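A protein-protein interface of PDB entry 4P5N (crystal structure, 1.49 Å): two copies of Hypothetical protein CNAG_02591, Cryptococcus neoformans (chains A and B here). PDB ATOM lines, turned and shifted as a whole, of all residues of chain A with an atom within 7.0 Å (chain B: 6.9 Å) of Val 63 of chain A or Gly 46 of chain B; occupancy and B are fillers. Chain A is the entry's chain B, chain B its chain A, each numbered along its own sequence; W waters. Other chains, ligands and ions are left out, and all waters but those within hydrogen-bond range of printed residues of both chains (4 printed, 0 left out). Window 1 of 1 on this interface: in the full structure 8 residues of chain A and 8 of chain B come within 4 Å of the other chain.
Ala 43 of chain B touches Tyr 23 of chain A.
OH of Tyr 23 of chain A touches CA of Glu 44 of chain B, at 3.6 Å.
Glu 44 of chain B touches His 28 of chain A.
His 28 of chain A touches Gly 46 of chain B.
Lys 45 of chain B touches Lys 61 of chain A.
Val 63 of chain A touches Gly 46 of chain B.
Water W3 lies within hydrogen-bond range of O of Lys 45 of chain B and O of Asp 62 of chain A.
Water W4 lies within hydrogen-bond range of the backbone carbonyl oxygen (O) of Gly 46 of chain B and the backbone NH (N) of Ala 64 of chain A.
Water W1 lies within hydrogen-bond range of the side-chain carboxylate of Asp 57 of chain A (2.8 Å) and the backbone carbonyl oxygen of Glu 44 of chain B (3.1 Å).
Water W2 lies within hydrogen-bond range of a ring nitrogen (NE2) of His 28 of chain A and the backbone carbonyl oxygen of Ala 43 of chain B.
2 positions are printed for both chains.
Of the 7 pairs that touch across the chains among the printed residues, none has its exchanged pair printed and touching as well.
Of the 17 printed residues of chain A, 4 touch a printed residue of chain B.
Printed residues of chain B that touch a printed residue of chain A: Ala 43, Glu 44, Lys 45 and Gly 46.
Among the printed residues, 7 pairs touch across the chains.
Among the printed residues, no Asp or Glu carboxylate lies within 4 Å of a Lys or Arg side-chain nitrogen of the other chain.
NE2 of His 28 of chain A lies within hydrogen-bond range of O of Ala 43 of chain B (2.7 Å).
Val 63 of chain A touches one residue of chain B.
Of chain A, only His 28 (3.5 Å) and Val 63 (3.9 Å) come within 4 Å of Gly 46 of chain B.
Printed residues of chain A within 4 Å of Ala 43 of chain B: Tyr 23 (3.6 Å) and His 28 (2.7 Å).
Of the printed residues of chain A, Glu 44 of chain B touches Tyr 23 and His 28.
Of the printed residues of chain B, Lys 61 of chain A touches Lys 45 (3.8 Å).
Printed residues of chain B within 4 Å of Tyr 23 of chain A: Ala 43 and Glu 44.
Of the printed residues of chain B, His 28 of chain A touches Ala 43, Glu 44 and Gly 46.
Thr 21 of chain A touches none of the printed residues of chain B.
The nearest printed residue of chain B that does not touch Val 63 of chain A is Lys 45 of chain B (5.0 Å).
The nearest residue of chain A that does not touch Gly 46 of chain B is Ala 64 of chain A (4.7 Å).
The nearest printed residue of chain B that does not touch Lys 61 of chain A is Glu 44 of chain B (4.2 Å).
The side-chain amino group (NZ) of Lys 45 of chain B lies close to the side-chain carboxylate (OE1) of Glu 41 of chain B (3.5 Å).
The backbone carbonyl oxygen (O) of Thr 21 of chain A sits at hydrogen-bond distance from the backbone NH (N) of His 28 of chain A.
A ring nitrogen (ND1) of His 28 of chain A is in hydrogen-bond range of the side-chain carboxylate of Asp 57 of chain A (2.7 Å).
N of Val 63 of chain A lies within hydrogen-bond range of O of Phe 55 of chain A (2.7 Å).
The backbone NH (N) of Lys 61 of chain A sits at hydrogen-bond distance from the side-chain carboxylate (OD1) of Asp 57 of chain A (2.9 Å).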
ATOM      1  N   THR A  21       0.292 -24.952  20.221  1.00  0.00           N
ATOM      2  CA  THR A  21      -0.272 -26.293  20.046  1.00  0.00           C
ATOM      3  C   THR A  21      -0.996 -26.333  18.711  1.00  0.00           C
ATOM      4  O   THR A  21      -1.759 -25.421  18.403  1.00  0.00           O
ATOM      5  CB  THR A  21      -1.203 -26.688  21.223  1.00  0.00           C
ATOM      6  OG1 THR A  21      -1.756 -27.987  20.974  1.00  0.00           O
ATOM      7  CG2 THR A  21      -2.331 -25.684  21.426  1.00  0.00           C
ATOM      8  N   TYR A  23      -3.622 -28.079  15.800  1.00  0.00           N
ATOM      9  CA  TYR A  23      -4.780 -28.967  15.641  1.00  0.00           C
ATOM     10  C   TYR A  23      -5.064 -29.141  14.155  1.00  0.00           C
ATOM     11  O   TYR A  23      -4.438 -28.481  13.321  1.00  0.00           O
ATOM     12  CB  TYR A  23      -6.022 -28.462  16.416  1.00  0.00           C
ATOM     13  CG  TYR A  23      -6.608 -27.175  15.878  1.00  0.00           C
ATOM     14  CD1 TYR A  23      -7.582 -27.201  14.874  1.00  0.00           C
ATOM     15  CD2 TYR A  23      -6.167 -25.932  16.341  1.00  0.00           C
ATOM     16  CE1 TYR A  23      -8.119 -26.035  14.347  1.00  0.00           C
ATOM     17  CE2 TYR A  23      -6.709 -24.752  15.830  1.00  0.00           C
ATOM     18  CZ  TYR A  23      -7.687 -24.810  14.843  1.00  0.00           C
ATOM     19  OH  TYR A  23      -8.224 -23.661  14.316  1.00  0.00           O
ATOM     20  N   HIS A  28      -3.077 -22.956  17.958  1.00  0.00           N
ATOM     21  CA  HIS A  28      -3.252 -21.937  19.007  1.00  0.00           C
ATOM     22  C   HIS A  28      -1.875 -21.530  19.485  1.00  0.00           C
ATOM     23  O   HIS A  28      -1.134 -22.347  20.022  1.00  0.00           O
ATOM     24  CB  HIS A  28      -4.074 -22.459  20.180  1.00  0.00           C
ATOM     25  CG  HIS A  28      -5.408 -22.976  19.765  1.00  0.00           C
ATOM     26  ND1 HIS A  28      -6.434 -22.143  19.366  1.00  0.00           N
ATOM     27  CD2 HIS A  28      -5.883 -24.242  19.653  1.00  0.00           C
ATOM     28  CE1 HIS A  28      -7.476 -22.876  19.008  1.00  0.00           C
ATOM     29  NE2 HIS A  28      -7.173 -24.153  19.189  1.00  0.00           N
ATOM     30  N   GLU A  29      -1.530 -20.269  19.255  1.00  0.00           N
ATOM     31  CA  GLU A  29      -0.229 -19.763  19.615  1.00  0.00           C
ATOM     32  C   GLU A  29      -0.401 -18.413  20.283  1.00  0.00           C
ATOM     33  O   GLU A  29      -1.147 -17.569  19.776  1.00  0.00           O
ATOM     34  CB  GLU A  29       0.600 -19.597  18.345  1.00  0.00           C
ATOM     35  CG  GLU A  29       2.001 -19.073  18.612  1.00  0.00           C
ATOM     36  CD  GLU A  29       2.815 -18.921  17.349  1.00  0.00           C
ATOM     37  OE1 GLU A  29       2.687 -19.786  16.454  1.00  0.00           O
ATOM     38  OE2 GLU A  29       3.563 -17.916  17.265  1.00  0.00           O
ATOM     39  N   VAL A  47     -11.306 -23.369  35.270  1.00  0.00           N
ATOM     40  CA  VAL A  47     -10.608 -24.444  34.578  1.00  0.00           C
ATOM     41  C   VAL A  47     -10.498 -25.650  35.516  1.00  0.00           C
ATOM     42  O   VAL A  47     -10.805 -25.541  36.714  1.00  0.00           O
ATOM     43  CB  VAL A  47      -9.245 -23.989  33.966  1.00  0.00           C
ATOM     44  CG1 VAL A  47      -9.477 -22.881  32.944  1.00  0.00           C
ATOM     45  CG2 VAL A  47      -8.247 -23.550  35.036  1.00  0.00           C
ATOM     46  N   VAL A  53      -1.799 -23.890  31.617  1.00  0.00           N
ATOM     47  CA  VAL A  53      -1.277 -22.602  31.192  1.00  0.00           C
ATOM     48  C   VAL A  53      -2.378 -21.896  30.423  1.00  0.00           C
ATOM     49  O   VAL A  53      -3.090 -22.477  29.585  1.00  0.00           O
ATOM     50  CB  VAL A  53       0.041 -22.665  30.389  1.00  0.00           C
ATOM     51  CG1 VAL A  53       1.208 -23.075  31.284  1.00  0.00           C
ATOM     52  CG2 VAL A  53      -0.085 -23.571  29.174  1.00  0.00           C
ATOM     53  N   LEU A  54      -2.548 -20.629  30.772  1.00  0.00           N
ATOM     54  CA  LEU A  54      -3.607 -19.818  30.199  1.00  0.00           C
ATOM     55  C   LEU A  54      -2.969 -18.815  29.242  1.00  0.00           C
ATOM     56  O   LEU A  54      -2.018 -18.124  29.608  1.00  0.00           O
ATOM     57  CB  LEU A  54      -4.378 -19.105  31.310  1.00  0.00           C
ATOM     58  CG  LEU A  54      -5.472 -19.919  32.035  1.00  0.00           C
ATOM     59  CD1 LEU A  54      -5.155 -21.334  32.492  1.00  0.00           C
ATOM     60  CD2 LEU A  54      -6.066 -19.080  33.167  1.00  0.00           C
ATOM     61  N   PHE A  55      -3.483 -18.745  28.020  1.00  0.00           N
ATOM     62  CA  PHE A  55      -2.980 -17.800  27.033  1.00  0.00           C
ATOM     63  C   PHE A  55      -4.094 -17.415  26.075  1.00  0.00           C
ATOM     64  O   PHE A  55      -5.059 -18.161  25.884  1.00  0.00           O
ATOM     65  CB  PHE A  55      -1.746 -18.340  26.267  1.00  0.00           C
ATOM     66  CG  PHE A  55      -2.016 -19.538  25.378  1.00  0.00           C
ATOM     67  CD1 PHE A  55      -2.112 -20.816  25.914  1.00  0.00           C
ATOM     68  CD2 PHE A  55      -2.108 -19.386  24.005  1.00  0.00           C
ATOM     69  CE1 PHE A  55      -2.323 -21.925  25.087  1.00  0.00           C
ATOM     70  CE2 PHE A  55      -2.314 -20.480  23.164  1.00  0.00           C
ATOM     71  CZ  PHE A  55      -2.424 -21.751  23.705  1.00  0.00           C
ATOM     72  N   THR A  56      -3.940 -16.244  25.468  1.00  0.00           N
ATOM     73  CA  THR A  56      -4.830 -15.811  24.415  1.00  0.00           C
ATOM     74  C   THR A  56      -4.143 -16.081  23.087  1.00  0.00           C
ATOM     75  O   THR A  56      -2.971 -15.719  22.896  1.00  0.00           O
ATOM     76  CB  THR A  56      -5.173 -14.320  24.582  1.00  0.00           C
ATOM     77  OG1 THR A  56      -5.861 -14.142  25.831  1.00  0.00           O
ATOM     78  CG2 THR A  56      -6.054 -13.839  23.437  1.00  0.00           C
ATOM     79  N   ASP A  57      -4.841 -16.761  22.182  1.00  0.00           N
ATOM     80  CA  ASP A  57      -4.199 -17.142  20.941  1.00  0.00           C
ATOM     81  C   ASP A  57      -4.245 -16.012  19.912  1.00  0.00           C
ATOM     82  O   ASP A  57      -4.690 -14.890  20.216  1.00  0.00           O
ATOM     83  CB  ASP A  57      -4.741 -18.487  20.410  1.00  0.00           C
ATOM     84  CG  ASP A  57      -6.100 -18.384  19.729  1.00  0.00           C
ATOM     85  OD1 ASP A  57      -6.649 -17.272  19.519  1.00  0.00           O
ATOM     86  OD2 ASP A  57      -6.607 -19.466  19.361  1.00  0.00           O
ATOM     87  N   ASN A  60      -7.510 -14.186  19.381  1.00  0.00           N
ATOM     88  CA  ASN A  60      -8.165 -13.703  20.601  1.00  0.00           C
ATOM     89  C   ASN A  60      -9.065 -14.722  21.316  1.00  0.00           C
ATOM     90  O   ASN A  60     -10.001 -14.341  22.037  1.00  0.00           O
ATOM     91  CB  ASN A  60      -8.856 -12.350  20.347  1.00  0.00           C
ATOM     92  CG  ASN A  60      -7.852 -11.245  20.150  1.00  0.00           C
ATOM     93  OD1 ASN A  60      -6.805 -11.252  20.792  1.00  0.00           O
ATOM     94  ND2 ASN A  60      -8.145 -10.300  19.257  1.00  0.00           N
ATOM     95  N   LYS A  61      -8.738 -16.009  21.175  1.00  0.00           N
ATOM     96  CA  LYS A  61      -9.426 -17.052  21.944  1.00  0.00           C
ATOM     97  C   LYS A  61      -8.645 -17.311  23.228  1.00  0.00           C
ATOM     98  O   LYS A  61      -7.430 -17.491  23.181  1.00  0.00           O
ATOM     99  CB  LYS A  61      -9.565 -18.354  21.129  1.00  0.00           C
ATOM    100  CG  LYS A  61     -10.180 -18.195  19.745  1.00  0.00           C
ATOM    101  CD  LYS A  61     -11.534 -17.513  19.820  1.00  0.00           C
ATOM    102  CE  LYS A  61     -12.217 -17.489  18.471  1.00  0.00           C
ATOM    103  NZ  LYS A  61     -13.507 -16.757  18.574  1.00  0.00           N
ATOM    104  N   ASP A  62      -9.316 -17.268  24.376  1.00  0.00           N
ATOM    105  CA  ASP A  62      -8.656 -17.615  25.637  1.00  0.00           C
ATOM    106  C   ASP A  62      -8.592 -19.134  25.721  1.00  0.00           C
ATOM    107  O   ASP A  62      -9.630 -19.824  25.685  1.00  0.00           O
ATOM    108  CB  ASP A  62      -9.396 -17.036  26.851  1.00  0.00           C
ATOM    109  CG  ASP A  62      -9.207 -15.523  27.001  1.00  0.00           C
ATOM    110  OD1 ASP A  62      -8.539 -14.874  26.162  1.00  0.00           O
ATOM    111  OD2 ASP A  62      -9.754 -14.947  27.966  1.00  0.00           O
ATOM    112  N   VAL A  63      -7.368 -19.642  25.792  1.00  0.00           N
ATOM    113  CA  VAL A  63      -7.103 -21.071  25.824  1.00  0.00           C
ATOM    114  C   VAL A  63      -6.518 -21.463  27.189  1.00  0.00           C
ATOM    115  O   VAL A  63      -5.674 -20.746  27.745  1.00  0.00           O
ATOM    116  CB  VAL A  63      -6.119 -21.463  24.697  1.00  0.00           C
ATOM    117  CG1 VAL A  63      -5.845 -22.952  24.707  1.00  0.00           C
ATOM    118  CG2 VAL A  63      -6.655 -21.052  23.335  1.00  0.00           C
ATOM    119  N   ALA A  64      -6.995 -22.577  27.739  1.00  0.00           N
ATOM    120  CA  ALA A  64      -6.366 -23.196  28.904  1.00  0.00           C
ATOM    121  C   ALA A  64      -5.895 -24.567  28.452  1.00  0.00           C
ATOM    122  O   ALA A  64      -6.679 -25.355  27.895  1.00  0.00           O
ATOM    123  CB  ALA A  64      -7.360 -23.322  30.045  1.00  0.00           C
ATOM    124  N   HIS A  65      -4.623 -24.853  28.677  1.00  0.00           N
ATOM    125  CA  HIS A  65      -4.019 -26.048  28.104  1.00  0.00           C
ATOM    126  C   HIS A  65      -3.067 -26.709  29.077  1.00  0.00           C
ATOM    127  O   HIS A  65      -2.367 -26.049  29.846  1.00  0.00           O
ATOM    128  CB  HIS A  65      -3.248 -25.671  26.828  1.00  0.00           C
ATOM    129  CG  HIS A  65      -3.126 -26.776  25.813  1.00  0.00           C
ATOM    130  ND1 HIS A  65      -2.196 -27.791  25.913  1.00  0.00           N
ATOM    131  CD2 HIS A  65      -3.773 -26.976  24.640  1.00  0.00           C
ATOM    132  CE1 HIS A  65      -2.284 -28.574  24.852  1.00  0.00           C
ATOM    133  NE2 HIS A  65      -3.241 -28.107  24.067  1.00  0.00           N
ATOM    134  N   LEU A  70       2.004 -29.089  25.180  1.00  0.00           N
ATOM    135  CA  LEU A  70       2.290 -28.045  24.193  1.00  0.00           C
ATOM    136  C   LEU A  70       3.788 -27.676  24.147  1.00  0.00           C
ATOM    137  O   LEU A  70       4.592 -28.237  24.900  1.00  0.00           O
ATOM    138  CB  LEU A  70       1.360 -26.824  24.385  1.00  0.00           C
ATOM    139  CG  LEU A  70       1.255 -26.146  25.749  1.00  0.00           C
ATOM    140  CD1 LEU A  70       2.606 -25.604  26.166  1.00  0.00           C
ATOM    141  CD2 LEU A  70       0.215 -25.043  25.669  1.00  0.00           C
ATOM    142  N   GLU B  41     -15.340 -27.266  15.665  1.00  0.00           N
ATOM    143  CA  GLU B  41     -15.545 -25.957  16.264  1.00  0.00           C
ATOM    144  C   GLU B  41     -14.851 -25.865  17.621  1.00  0.00           C
ATOM    145  O   GLU B  41     -14.303 -24.820  17.981  1.00  0.00           O
ATOM    146  CB  GLU B  41     -17.028 -25.709  16.440  1.00  0.00           C
ATOM    147  CG  GLU B  41     -17.406 -24.288  16.777  1.00  0.00           C
ATOM    148  CD  GLU B  41     -18.886 -24.161  17.102  1.00  0.00           C
ATOM    149  OE1 GLU B  41     -19.294 -23.041  17.445  1.00  0.00           O
ATOM    150  OE2 GLU B  41     -19.644 -25.175  17.029  1.00  0.00           O
ATOM    151  N   ALA B  42     -14.862 -26.958  18.373  1.00  0.00           N
ATOM    152  CA  ALA B  42     -14.176 -26.986  19.660  1.00  0.00           C
ATOM    153  C   ALA B  42     -12.682 -26.746  19.475  1.00  0.00           C
ATOM    154  O   ALA B  42     -12.073 -25.956  20.205  1.00  0.00           O
ATOM    155  CB  ALA B  42     -14.439 -28.301  20.393  1.00  0.00           C
ATOM    156  N   ALA B  43     -12.103 -27.419  18.487  1.00  0.00           N
ATOM    157  CA  ALA B  43     -10.697 -27.242  18.184  1.00  0.00           C
ATOM    158  C   ALA B  43     -10.394 -25.793  17.802  1.00  0.00           C
ATOM    159  O   ALA B  43      -9.442 -25.205  18.306  1.00  0.00           O
ATOM    160  CB  ALA B  43     -10.257 -28.200  17.092  1.00  0.00           C
ATOM    161  N   GLU B  44     -11.217 -25.216  16.932  1.00  0.00           N
ATOM    162  CA  GLU B  44     -11.027 -23.829  16.520  1.00  0.00           C
ATOM    163  C   GLU B  44     -11.094 -22.836  17.696  1.00  0.00           C
ATOM    164  O   GLU B  44     -10.352 -21.865  17.721  1.00  0.00           O
ATOM    165  CB  GLU B  44     -12.033 -23.445  15.441  1.00  0.00           C
ATOM    166  CG  GLU B  44     -11.938 -21.993  15.003  1.00  0.00           C
ATOM    167  CD  GLU B  44     -13.052 -21.599  14.063  1.00  0.00           C
ATOM    168  OE1 GLU B  44     -14.230 -21.842  14.402  1.00  0.00           O
ATOM    169  OE2 GLU B  44     -12.746 -21.037  12.993  1.00  0.00           O
ATOM    170  N   LYS B  45     -11.974 -23.105  18.658  1.00  0.00           N
ATOM    171  CA  LYS B  45     -12.173 -22.217  19.802  1.00  0.00           C
ATOM    172  C   LYS B  45     -11.268 -22.571  20.986  1.00  0.00           C
ATOM    173  O   LYS B  45     -11.374 -21.961  22.052  1.00  0.00           O
ATOM    174  CB  LYS B  45     -13.644 -22.221  20.230  1.00  0.00           C
ATOM    175  CG  LYS B  45     -14.617 -21.889  19.108  1.00  0.00           C
ATOM    176  CD  LYS B  45     -14.602 -20.414  18.742  1.00  0.00           C
ATOM    177  CE  LYS B  45     -15.280 -20.164  17.399  1.00  0.00           C
ATOM    178  NZ  LYS B  45     -16.696 -20.638  17.356  1.00  0.00           N
ATOM    179  N   GLY B  46     -10.389 -23.555  20.798  1.00  0.00           N
ATOM    180  CA  GLY B  46      -9.413 -23.934  21.815  1.00  0.00           C
ATOM    181  C   GLY B  46      -9.965 -24.639  23.035  1.00  0.00           C
ATOM    182  O   GLY B  46      -9.357 -24.593  24.095  1.00  0.00           O
ATOM    183  N   VAL B  47     -11.121 -25.281  22.882  1.00  0.00           N
ATOM    184  CA  VAL B  47     -11.750 -26.020  23.976  1.00  0.00           C
ATOM    185  C   VAL B  47     -11.834 -27.496  23.615  1.00  0.00           C
ATOM    186  O   VAL B  47     -11.534 -27.869  22.486  1.00  0.00           O
ATOM    187  CB  VAL B  47     -13.136 -25.448  24.380  1.00  0.00           C
ATOM    188  CG1 VAL B  47     -12.996 -23.979  24.776  1.00  0.00           C
ATOM    189  CG2 VAL B  47     -14.160 -25.595  23.266  1.00  0.00           C
ATOM    190  N   LYS B  48     -12.239 -28.318  24.576  1.00  0.00           N
ATOM    191  CA  LYS B  48     -12.277 -29.769  24.399  1.00  0.00           C
ATOM    192  C   LYS B  48     -13.642 -30.304  24.764  1.00  0.00           C
ATOM    193  O   LYS B  48     -14.373 -29.684  25.559  1.00  0.00           O
ATOM    194  CB  LYS B  48     -11.242 -30.446  25.296  1.00  0.00           C
ATOM    195  CG  LYS B  48      -9.797 -30.089  24.995  1.00  0.00           C
ATOM    196  CD  LYS B  48      -8.849 -30.656  26.040  1.00  0.00           C
ATOM    197  CE  LYS B  48      -8.482 -32.098  25.735  1.00  0.00           C
ATOM    198  NZ  LYS B  48      -7.197 -32.435  26.397  1.00  0.00           N
ATOM    199  N   ALA B  64     -15.439 -22.220  29.717  1.00  0.00           N
ATOM    200  CA  ALA B  64     -16.063 -23.168  28.793  1.00  0.00           C
ATOM    201  C   ALA B  64     -16.604 -24.313  29.637  1.00  0.00           C
ATOM    202  O   ALA B  64     -15.824 -25.002  30.328  1.00  0.00           O
ATOM    203  CB  ALA B  64     -15.050 -23.684  27.780  1.00  0.00           C
HETATM  204  O   HOH W   1      -8.138 -19.753  17.090  1.00  0.00           O
HETATM  205  O   HOH W   2      -7.174 -27.273  19.639  1.00  0.00           O
HETATM  206  O   HOH W   3     -11.935 -20.037  23.928  1.00  0.00           O
HETATM  207  O   HOH W   4      -9.487 -23.694  26.690  1.00  0.00           O
